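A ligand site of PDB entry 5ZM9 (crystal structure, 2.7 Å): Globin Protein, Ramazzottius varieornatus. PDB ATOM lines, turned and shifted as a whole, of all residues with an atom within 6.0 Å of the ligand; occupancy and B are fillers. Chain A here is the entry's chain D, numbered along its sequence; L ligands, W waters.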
ATOM      1  N   LEU A  53      -9.257 -24.845 -16.738  1.00  0.00           N
ATOM      2  CA  LEU A  53      -8.388 -24.201 -17.729  1.00  0.00           C
ATOM      3  C   LEU A  53      -7.784 -22.914 -17.170  1.00  0.00           C
ATOM      4  O   LEU A  53      -6.603 -22.656 -17.382  1.00  0.00           O
ATOM      5  CB  LEU A  53      -9.155 -23.929 -19.033  1.00  0.00           C
ATOM      6  CG  LEU A  53      -8.352 -23.532 -20.276  1.00  0.00           C
ATOM      7  CD1 LEU A  53      -7.765 -24.749 -20.988  1.00  0.00           C
ATOM      8  CD2 LEU A  53      -9.216 -22.731 -21.235  1.00  0.00           C
ATOM      9  N   PHE A  54      -8.592 -22.130 -16.455  1.00  0.00           N
ATOM     10  CA  PHE A  54      -8.148 -20.876 -15.849  1.00  0.00           C
ATOM     11  C   PHE A  54      -7.272 -21.068 -14.609  1.00  0.00           C
ATOM     12  O   PHE A  54      -6.445 -20.212 -14.295  1.00  0.00           O
ATOM     13  CB  PHE A  54      -9.334 -19.947 -15.538  1.00  0.00           C
ATOM     14  CG  PHE A  54     -10.098 -19.487 -16.761  1.00  0.00           C
ATOM     15  CD1 PHE A  54      -9.456 -19.235 -17.974  1.00  0.00           C
ATOM     16  CD2 PHE A  54     -11.475 -19.258 -16.676  1.00  0.00           C
ATOM     17  CE1 PHE A  54     -10.174 -18.805 -19.096  1.00  0.00           C
ATOM     18  CE2 PHE A  54     -12.195 -18.816 -17.786  1.00  0.00           C
ATOM     19  CZ  PHE A  54     -11.543 -18.594 -18.990  1.00  0.00           C
ATOM     20  N   MET A  60      -4.719 -18.107 -20.080  1.00  0.00           N
ATOM     21  CA  MET A  60      -5.943 -18.285 -20.871  1.00  0.00           C
ATOM     22  C   MET A  60      -7.075 -17.348 -20.429  1.00  0.00           C
ATOM     23  O   MET A  60      -8.028 -17.126 -21.193  1.00  0.00           O
ATOM     24  CB  MET A  60      -6.416 -19.746 -20.814  1.00  0.00           C
ATOM     25  CG  MET A  60      -5.394 -20.796 -21.250  1.00  0.00           C
ATOM     26  SD  MET A  60      -5.171 -20.996 -23.028  1.00  0.00           S
ATOM     27  CE  MET A  60      -4.000 -19.703 -23.415  1.00  0.00           C
ATOM     28  N   LYS A  61      -6.949 -16.817 -19.220  1.00  0.00           N
ATOM     29  CA  LYS A  61      -7.908 -15.870 -18.625  1.00  0.00           C
ATOM     30  C   LYS A  61      -7.953 -14.528 -19.360  1.00  0.00           C
ATOM     31  O   LYS A  61      -8.981 -13.850 -19.346  1.00  0.00           O
ATOM     32  CB  LYS A  61      -7.560 -15.653 -17.153  1.00  0.00           C
ATOM     33  CG  LYS A  61      -8.772 -15.451 -16.244  1.00  0.00           C
ATOM     34  CD  LYS A  61      -8.352 -15.305 -14.783  1.00  0.00           C
ATOM     35  CE  LYS A  61      -8.097 -16.649 -14.097  1.00  0.00           C
ATOM     36  NZ  LYS A  61      -7.749 -16.491 -12.664  1.00  0.00           N
ATOM     37  N   LEU A  63      -7.680 -13.997 -22.627  1.00  0.00           N
ATOM     38  CA  LEU A  63      -8.442 -14.136 -23.865  1.00  0.00           C
ATOM     39  C   LEU A  63      -9.925 -13.826 -23.640  1.00  0.00           C
ATOM     40  O   LEU A  63     -10.634 -13.425 -24.574  1.00  0.00           O
ATOM     41  CB  LEU A  63      -8.267 -15.543 -24.464  1.00  0.00           C
ATOM     42  CG  LEU A  63      -6.966 -15.878 -25.211  1.00  0.00           C
ATOM     43  CD1 LEU A  63      -5.841 -16.294 -24.272  1.00  0.00           C
ATOM     44  CD2 LEU A  63      -7.226 -16.975 -26.215  1.00  0.00           C
ATOM     45  N   PHE A  64     -10.373 -14.007 -22.395  1.00  0.00           N
ATOM     46  CA  PHE A  64     -11.699 -13.600 -21.936  1.00  0.00           C
ATOM     47  C   PHE A  64     -11.529 -12.486 -20.891  1.00  0.00           C
ATOM     48  O   PHE A  64     -11.519 -12.782 -19.688  1.00  0.00           O
ATOM     49  CB  PHE A  64     -12.446 -14.782 -21.326  1.00  0.00           C
ATOM     50  CG  PHE A  64     -12.697 -15.932 -22.262  1.00  0.00           C
ATOM     51  CD1 PHE A  64     -13.818 -15.925 -23.103  1.00  0.00           C
ATOM     52  CD2 PHE A  64     -11.835 -17.034 -22.289  1.00  0.00           C
ATOM     53  CE1 PHE A  64     -14.062 -16.993 -23.963  1.00  0.00           C
ATOM     54  CE2 PHE A  64     -12.080 -18.103 -23.148  1.00  0.00           C
ATOM     55  CZ  PHE A  64     -13.186 -18.082 -23.984  1.00  0.00           C
ATOM     56  N   ALA A  87     -20.564 -22.919 -24.537  1.00  0.00           N
ATOM     57  CA  ALA A  87     -20.033 -22.878 -25.905  1.00  0.00           C
ATOM     58  C   ALA A  87     -18.772 -23.741 -26.093  1.00  0.00           C
ATOM     59  O   ALA A  87     -18.360 -24.004 -27.235  1.00  0.00           O
ATOM     60  CB  ALA A  87     -19.771 -21.444 -26.336  1.00  0.00           C
ATOM     61  N   HIS A  88     -18.210 -24.207 -24.998  1.00  0.00           N
ATOM     62  CA  HIS A  88     -17.004 -25.019 -24.995  1.00  0.00           C
ATOM     63  C   HIS A  88     -17.224 -26.481 -24.672  1.00  0.00           C
ATOM     64  O   HIS A  88     -16.389 -27.324 -24.991  1.00  0.00           O
ATOM     65  CB  HIS A  88     -15.971 -24.403 -24.054  1.00  0.00           C
ATOM     66  CG  HIS A  88     -15.254 -23.249 -24.666  1.00  0.00           C
ATOM     67  ND1 HIS A  88     -15.643 -21.956 -24.475  1.00  0.00           N
ATOM     68  CD2 HIS A  88     -14.243 -23.225 -25.542  1.00  0.00           C
ATOM     69  CE1 HIS A  88     -14.875 -21.173 -25.190  1.00  0.00           C
ATOM     70  NE2 HIS A  88     -14.034 -21.911 -25.879  1.00  0.00           N
ATOM     71  N   ILE A  89     -18.375 -26.755 -24.068  1.00  0.00           N
ATOM     72  CA  ILE A  89     -18.773 -28.118 -23.715  1.00  0.00           C
ATOM     73  C   ILE A  89     -19.717 -28.757 -24.750  1.00  0.00           C
ATOM     74  O   ILE A  89     -19.679 -29.979 -24.951  1.00  0.00           O
ATOM     75  CB  ILE A  89     -19.330 -28.201 -22.256  1.00  0.00           C
ATOM     76  CG1 ILE A  89     -19.294 -29.637 -21.704  1.00  0.00           C
ATOM     77  CG2 ILE A  89     -20.723 -27.587 -22.119  1.00  0.00           C
ATOM     78  CD1 ILE A  89     -18.045 -29.966 -20.918  1.00  0.00           C
ATOM     79  N   PRO A  91     -19.735 -28.468 -28.183  1.00  0.00           N
ATOM     80  CA  PRO A  91     -19.095 -29.173 -29.308  1.00  0.00           C
ATOM     81  C   PRO A  91     -18.709 -30.623 -28.979  1.00  0.00           C
ATOM     82  O   PRO A  91     -18.781 -31.482 -29.866  1.00  0.00           O
ATOM     83  CB  PRO A  91     -17.848 -28.343 -29.575  1.00  0.00           C
ATOM     84  CG  PRO A  91     -18.221 -26.972 -29.149  1.00  0.00           C
ATOM     85  CD  PRO A  91     -19.055 -27.181 -27.918  1.00  0.00           C
ATOM     86  N   TYR A  92     -18.314 -30.888 -27.731  1.00  0.00           N
ATOM     87  CA  TYR A  92     -18.036 -32.245 -27.250  1.00  0.00           C
ATOM     88  C   TYR A  92     -19.307 -33.086 -27.148  1.00  0.00           C
ATOM     89  O   TYR A  92     -19.277 -34.293 -27.400  1.00  0.00           O
ATOM     90  CB  TYR A  92     -17.308 -32.209 -25.901  1.00  0.00           C
ATOM     91  CG  TYR A  92     -15.873 -31.743 -25.952  1.00  0.00           C
ATOM     92  CD1 TYR A  92     -14.874 -32.518 -26.552  1.00  0.00           C
ATOM     93  CD2 TYR A  92     -15.507 -30.521 -25.361  1.00  0.00           C
ATOM     94  CE1 TYR A  92     -13.548 -32.082 -26.584  1.00  0.00           C
ATOM     95  CE2 TYR A  92     -14.181 -30.085 -25.393  1.00  0.00           C
ATOM     96  CZ  TYR A  92     -13.209 -30.873 -26.003  1.00  0.00           C
ATOM     97  OH  TYR A  92     -11.906 -30.444 -26.032  1.00  0.00           O
ATOM     98  N   VAL A 112     -14.981 -25.866 -35.283  1.00  0.00           N
ATOM     99  CA  VAL A 112     -14.617 -25.402 -33.937  1.00  0.00           C
ATOM    100  C   VAL A 112     -13.202 -24.825 -33.914  1.00  0.00           C
ATOM    101  O   VAL A 112     -12.993 -23.704 -33.443  1.00  0.00           O
ATOM    102  CB  VAL A 112     -14.828 -26.510 -32.870  1.00  0.00           C
ATOM    103  CG1 VAL A 112     -14.086 -26.195 -31.571  1.00  0.00           C
ATOM    104  CG2 VAL A 112     -16.309 -26.697 -32.581  1.00  0.00           C
ATOM    105  N   GLN A 115     -12.841 -21.417 -35.680  1.00  0.00           N
ATOM    106  CA  GLN A 115     -13.356 -20.240 -34.944  1.00  0.00           C
ATOM    107  C   GLN A 115     -12.252 -19.447 -34.241  1.00  0.00           C
ATOM    108  O   GLN A 115     -12.375 -18.236 -34.054  1.00  0.00           O
ATOM    109  CB  GLN A 115     -14.423 -20.640 -33.897  1.00  0.00           C
ATOM    110  CG  GLN A 115     -15.509 -21.609 -34.339  1.00  0.00           C
ATOM    111  CD  GLN A 115     -16.633 -20.963 -35.150  1.00  0.00           C
ATOM    112  OE1 GLN A 115     -16.406 -20.397 -36.219  1.00  0.00           O
ATOM    113  NE2 GLN A 115     -17.847 -21.073 -34.633  1.00  0.00           N
ATOM    114  N   HIS A 116     -11.191 -20.150 -33.852  1.00  0.00           N
ATOM    115  CA  HIS A 116     -10.108 -19.610 -33.035  1.00  0.00           C
ATOM    116  C   HIS A 116      -9.051 -18.814 -33.818  1.00  0.00           C
ATOM    117  O   HIS A 116      -8.164 -18.201 -33.220  1.00  0.00           O
ATOM    118  CB  HIS A 116      -9.455 -20.742 -32.233  1.00  0.00           C
ATOM    119  CG  HIS A 116     -10.398 -21.433 -31.300  1.00  0.00           C
ATOM    120  ND1 HIS A 116     -11.206 -22.470 -31.699  1.00  0.00           N
ATOM    121  CD2 HIS A 116     -10.674 -21.218 -29.994  1.00  0.00           C
ATOM    122  CE1 HIS A 116     -11.934 -22.872 -30.666  1.00  0.00           C
ATOM    123  NE2 HIS A 116     -11.622 -22.132 -29.628  1.00  0.00           N
ATOM    124  N   VAL A 119      -9.360 -15.090 -33.155  1.00  0.00           N
ATOM    125  CA  VAL A 119      -8.853 -14.755 -31.821  1.00  0.00           C
ATOM    126  C   VAL A 119      -7.366 -14.382 -31.924  1.00  0.00           C
ATOM    127  O   VAL A 119      -6.561 -15.187 -32.402  1.00  0.00           O
ATOM    128  CB  VAL A 119      -9.061 -15.907 -30.802  1.00  0.00           C
ATOM    129  CG1 VAL A 119      -8.702 -15.467 -29.387  1.00  0.00           C
ATOM    130  CG2 VAL A 119     -10.500 -16.411 -30.830  1.00  0.00           C
ATOM    131  N   PHE A 122      -3.807 -16.630 -30.825  1.00  0.00           N
ATOM    132  CA  PHE A 122      -4.195 -18.002 -30.513  1.00  0.00           C
ATOM    133  C   PHE A 122      -3.211 -18.996 -31.128  1.00  0.00           C
ATOM    134  O   PHE A 122      -2.830 -18.869 -32.294  1.00  0.00           O
ATOM    135  CB  PHE A 122      -5.628 -18.312 -30.972  1.00  0.00           C
ATOM    136  CG  PHE A 122      -6.259 -19.471 -30.244  1.00  0.00           C
ATOM    137  CD1 PHE A 122      -6.070 -20.782 -30.678  1.00  0.00           C
ATOM    138  CD2 PHE A 122      -7.051 -19.244 -29.115  1.00  0.00           C
ATOM    139  CE1 PHE A 122      -6.638 -21.848 -30.004  1.00  0.00           C
ATOM    140  CE2 PHE A 122      -7.635 -20.310 -28.434  1.00  0.00           C
ATOM    141  CZ  PHE A 122      -7.423 -21.614 -28.872  1.00  0.00           C
ATOM    142  N   TYR A 126      -2.829 -24.689 -27.702  1.00  0.00           N
ATOM    143  CA  TYR A 126      -3.833 -24.287 -26.708  1.00  0.00           C
ATOM    144  C   TYR A 126      -4.946 -25.315 -26.518  1.00  0.00           C
ATOM    145  O   TYR A 126      -5.415 -25.513 -25.397  1.00  0.00           O
ATOM    146  CB  TYR A 126      -4.439 -22.921 -27.077  1.00  0.00           C
ATOM    147  CG  TYR A 126      -3.576 -21.685 -26.823  1.00  0.00           C
ATOM    148  CD1 TYR A 126      -2.273 -21.788 -26.313  1.00  0.00           C
ATOM    149  CD2 TYR A 126      -4.074 -20.403 -27.122  1.00  0.00           C
ATOM    150  CE1 TYR A 126      -1.495 -20.646 -26.084  1.00  0.00           C
ATOM    151  CE2 TYR A 126      -3.301 -19.266 -26.906  1.00  0.00           C
ATOM    152  CZ  TYR A 126      -2.021 -19.391 -26.395  1.00  0.00           C
ATOM    153  OH  TYR A 126      -1.264 -18.269 -26.175  1.00  0.00           O
ATOM    154  N   PHE A 127      -5.347 -25.966 -27.620  1.00  0.00           N
ATOM    155  CA  PHE A 127      -6.446 -26.944 -27.617  1.00  0.00           C
ATOM    156  C   PHE A 127      -6.214 -28.168 -26.731  1.00  0.00           C
ATOM    157  O   PHE A 127      -7.158 -28.703 -26.131  1.00  0.00           O
ATOM    158  CB  PHE A 127      -6.757 -27.410 -29.054  1.00  0.00           C
ATOM    159  CG  PHE A 127      -7.285 -26.337 -29.957  1.00  0.00           C
ATOM    160  CD1 PHE A 127      -8.395 -25.565 -29.606  1.00  0.00           C
ATOM    161  CD2 PHE A 127      -6.680 -26.107 -31.204  1.00  0.00           C
ATOM    162  CE1 PHE A 127      -8.883 -24.572 -30.458  1.00  0.00           C
ATOM    163  CE2 PHE A 127      -7.167 -25.128 -32.058  1.00  0.00           C
ATOM    164  CZ  PHE A 127      -8.266 -24.358 -31.694  1.00  0.00           C
ATOM    165  N   GLU A 128      -4.950 -28.607 -26.647  1.00  0.00           N
ATOM    166  CA  GLU A 128      -4.550 -29.765 -25.833  1.00  0.00           C
ATOM    167  C   GLU A 128      -4.655 -29.525 -24.331  1.00  0.00           C
ATOM    168  O   GLU A 128      -4.711 -30.466 -23.543  1.00  0.00           O
ATOM    169  CB  GLU A 128      -3.133 -30.217 -26.201  1.00  0.00           C
ATOM    170  CG  GLU A 128      -2.862 -31.700 -25.970  1.00  0.00           C
ATOM    171  CD  GLU A 128      -1.381 -32.065 -25.921  1.00  0.00           C
ATOM    172  OE1 GLU A 128      -0.570 -31.447 -26.639  1.00  0.00           O
ATOM    173  OE2 GLU A 128      -1.023 -32.981 -25.145  1.00  0.00           O
ATOM    174  N   ARG A 129      -4.675 -28.241 -23.928  1.00  0.00           N
ATOM    175  CA  ARG A 129      -4.849 -27.856 -22.528  1.00  0.00           C
ATOM    176  C   ARG A 129      -6.247 -28.201 -22.000  1.00  0.00           C
ATOM    177  O   ARG A 129      -6.418 -28.417 -20.791  1.00  0.00           O
ATOM    178  CB  ARG A 129      -4.569 -26.358 -22.338  1.00  0.00           C
ATOM    179  CG  ARG A 129      -3.155 -25.927 -22.682  1.00  0.00           C
ATOM    180  CD  ARG A 129      -2.987 -24.427 -22.542  1.00  0.00           C
ATOM    181  NE  ARG A 129      -1.652 -23.978 -22.946  1.00  0.00           N
ATOM    182  CZ  ARG A 129      -1.114 -22.791 -22.660  1.00  0.00           C
ATOM    183  NH1 ARG A 129      -1.785 -21.895 -21.944  1.00  0.00           N
ATOM    184  NH2 ARG A 129       0.107 -22.503 -23.076  1.00  0.00           N
ATOM    185  N   MET A 130      -7.223 -28.272 -22.908  1.00  0.00           N
ATOM    186  CA  MET A 130      -8.631 -28.523 -22.577  1.00  0.00           C
ATOM    187  C   MET A 130      -8.962 -29.974 -22.220  1.00  0.00           C
ATOM    188  O   MET A 130      -9.853 -30.221 -21.396  1.00  0.00           O
ATOM    189  CB  MET A 130      -9.538 -28.023 -23.718  1.00  0.00           C
ATOM    190  CG  MET A 130     -11.012 -27.856 -23.355  1.00  0.00           C
ATOM    191  SD  MET A 130     -11.344 -26.525 -22.192  1.00  0.00           S
ATOM    192  CE  MET A 130     -11.416 -25.107 -23.289  1.00  0.00           C
ATOM    193  N   THR A 162      -9.344 -33.359 -30.094  1.00  0.00           N
ATOM    194  CA  THR A 162      -8.327 -32.306 -30.107  1.00  0.00           C
ATOM    195  C   THR A 162      -7.540 -32.284 -31.420  1.00  0.00           C
ATOM    196  O   THR A 162      -7.300 -31.209 -31.983  1.00  0.00           O
ATOM    197  CB  THR A 162      -7.350 -32.451 -28.907  1.00  0.00           C
ATOM    198  OG1 THR A 162      -8.103 -32.615 -27.699  1.00  0.00           O
ATOM    199  CG2 THR A 162      -6.450 -31.219 -28.768  1.00  0.00           C
ATOM    200  N   ILE A 165      -9.801 -30.831 -34.057  1.00  0.00           N
ATOM    201  CA  ILE A 165      -9.942 -29.398 -33.780  1.00  0.00           C
ATOM    202  C   ILE A 165      -8.675 -28.651 -34.252  1.00  0.00           C
ATOM    203  O   ILE A 165      -8.777 -27.596 -34.887  1.00  0.00           O
ATOM    204  CB  ILE A 165     -10.278 -29.125 -32.282  1.00  0.00           C
ATOM    205  CG1 ILE A 165     -11.708 -29.602 -31.970  1.00  0.00           C
ATOM    206  CG2 ILE A 165     -10.172 -27.649 -31.933  1.00  0.00           C
ATOM    207  CD1 ILE A 165     -11.978 -29.911 -30.509  1.00  0.00           C
HETATM  208  C1  LIG L   1     -14.585 -19.505 -29.363  1.00  0.00           C
HETATM  209  C2  LIG L   1     -15.184 -24.254 -28.537  1.00  0.00           C
HETATM  210  C3  LIG L   1     -10.630 -24.361 -26.795  1.00  0.00           C
HETATM  211  C4  LIG L   1     -10.894 -19.573 -26.226  1.00  0.00           C
HETATM  212  C5  LIG L   1     -15.084 -20.780 -29.390  1.00  0.00           C
HETATM  213  C6  LIG L   1     -16.239 -21.200 -30.104  1.00  0.00           C
HETATM  214  C7  LIG L   1     -16.413 -22.533 -29.876  1.00  0.00           C
HETATM  215  C8  LIG L   1     -15.362 -22.956 -29.021  1.00  0.00           C
HETATM  216  C9  LIG L   1     -17.522 -23.398 -30.434  1.00  0.00           C
HETATM  217  C10 LIG L   1     -17.120 -20.308 -30.951  1.00  0.00           C
HETATM  218  C11 LIG L   1     -18.108 -19.613 -30.014  1.00  0.00           C
HETATM  219  C12 LIG L   1     -19.294 -19.073 -30.774  1.00  0.00           C
HETATM  220  O1  LIG L   1     -20.373 -19.691 -30.744  1.00  0.00           O
HETATM  221  O2  LIG L   1     -19.193 -18.011 -31.427  1.00  0.00           O
HETATM  222  C13 LIG L   1     -13.954 -24.739 -28.050  1.00  0.00           C
HETATM  223  C14 LIG L   1     -13.623 -26.117 -27.861  1.00  0.00           C
HETATM  224  C15 LIG L   1     -12.348 -26.166 -27.372  1.00  0.00           C
HETATM  225  C16 LIG L   1     -11.898 -24.752 -27.264  1.00  0.00           C
HETATM  226  C17 LIG L   1     -14.515 -27.314 -28.138  1.00  0.00           C
HETATM  227  C18 LIG L   1     -11.558 -27.367 -27.024  1.00  0.00           C
HETATM  228  C19 LIG L   1     -10.585 -27.791 -27.820  1.00  0.00           C
HETATM  229  C20 LIG L   1     -10.285 -23.057 -26.418  1.00  0.00           C
HETATM  230  C21 LIG L   1      -9.141 -22.660 -25.699  1.00  0.00           C
HETATM  231  C22 LIG L   1      -9.225 -21.281 -25.540  1.00  0.00           C
HETATM  232  C23 LIG L   1     -10.423 -20.848 -26.162  1.00  0.00           C
HETATM  233  C24 LIG L   1      -8.028 -23.551 -25.210  1.00  0.00           C
HETATM  234  C25 LIG L   1      -8.243 -20.411 -24.858  1.00  0.00           C
HETATM  235  C26 LIG L   1      -8.556 -19.824 -23.695  1.00  0.00           C
HETATM  236  C27 LIG L   1     -11.904 -19.197 -27.108  1.00  0.00           C
HETATM  237  C28 LIG L   1     -12.140 -17.783 -27.403  1.00  0.00           C
HETATM  238  C29 LIG L   1     -13.172 -17.752 -28.269  1.00  0.00           C
HETATM  239  C30 LIG L   1     -13.545 -19.163 -28.502  1.00  0.00           C
HETATM  240  C31 LIG L   1     -11.366 -16.610 -26.815  1.00  0.00           C
HETATM  241  C32 LIG L   1     -13.828 -16.524 -28.901  1.00  0.00           C
HETATM  242  C33 LIG L   1     -14.602 -15.705 -27.858  1.00  0.00           C
HETATM  243  C34 LIG L   1     -15.899 -15.207 -28.424  1.00  0.00           C
HETATM  244  O3  LIG L   1     -16.970 -15.793 -28.136  1.00  0.00           O
HETATM  245  O4  LIG L   1     -15.918 -14.195 -29.158  1.00  0.00           O
HETATM  246  N1  LIG L   1     -14.579 -21.869 -28.715  1.00  0.00           N
HETATM  247  N2  LIG L   1     -12.904 -23.987 -27.681  1.00  0.00           N
HETATM  248  N3  LIG L   1     -11.056 -21.951 -26.660  1.00  0.00           N
HETATM  249  N4  LIG L   1     -12.761 -19.992 -27.777  1.00  0.00           N
HETATM  250 FE1  LIG L   1     -12.846 -21.889 -27.755  1.00  0.00          FE
HETATM  251  O   HOH W   1     -19.532 -16.774 -26.266  1.00  0.00           O
HETATM  252  O   HOH W   2     -16.999 -18.425 -26.137  1.00  0.00           O
HETATM  253  O   HOH W   3     -19.437 -13.772 -28.445  1.00  0.00           O
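An iron atom (FE1) of the ligand is bound by a ring nitrogen (NE2) of His 88 (2.2 Å).
NE2 of His 116 is bound to FE1 of the ligand (2.3 Å).
A ring nitrogen (ND1) of His 116 is in hydrogen-bond range of the backbone carbonyl oxygen of Val 112 (2.8 Å).
The side-chain sulfur (SD) of Met 60 lies close to the guanidinium group (NH1) of Arg 129.
Merely in contact with the ligand: Tyr 92 (3.3 Å), Tyr 126 (3.3 Å), Ala 87 (3.4 Å), Phe 122 (3.4 Å), Phe 64 (3.5 Å), Met 60 (3.6 Å), Phe 127 (3.6 Å), Val 112 (3.6 Å), Met 130 (3.7 Å), Ile 165 (3.7 Å), Pro 91 (3.8 Å), Gln 115 (3.8 Å), Leu 63 (3.8 Å), Val 119 (3.8 Å) and Leu 53 (3.9 Å).
Hydrophobic or aromatic side chains within 4 Å of the ligand: Leu 53, Met 60, Leu 63, Phe 64, His 88, Pro 91, Tyr 92, Val 112, His 116, Val 119, Phe 122, Phe 127, Met 130 and Ile 165.
17 residues have an atom within 4 Å of the ligand: Leu 53, Met 60, Leu 63, Phe 64, Ala 87, His 88, Pro 91, Tyr 92, Val 112, Gln 115, His 116, Val 119, Phe 122, Tyr 126, Phe 127, Met 130 and Ile 165.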
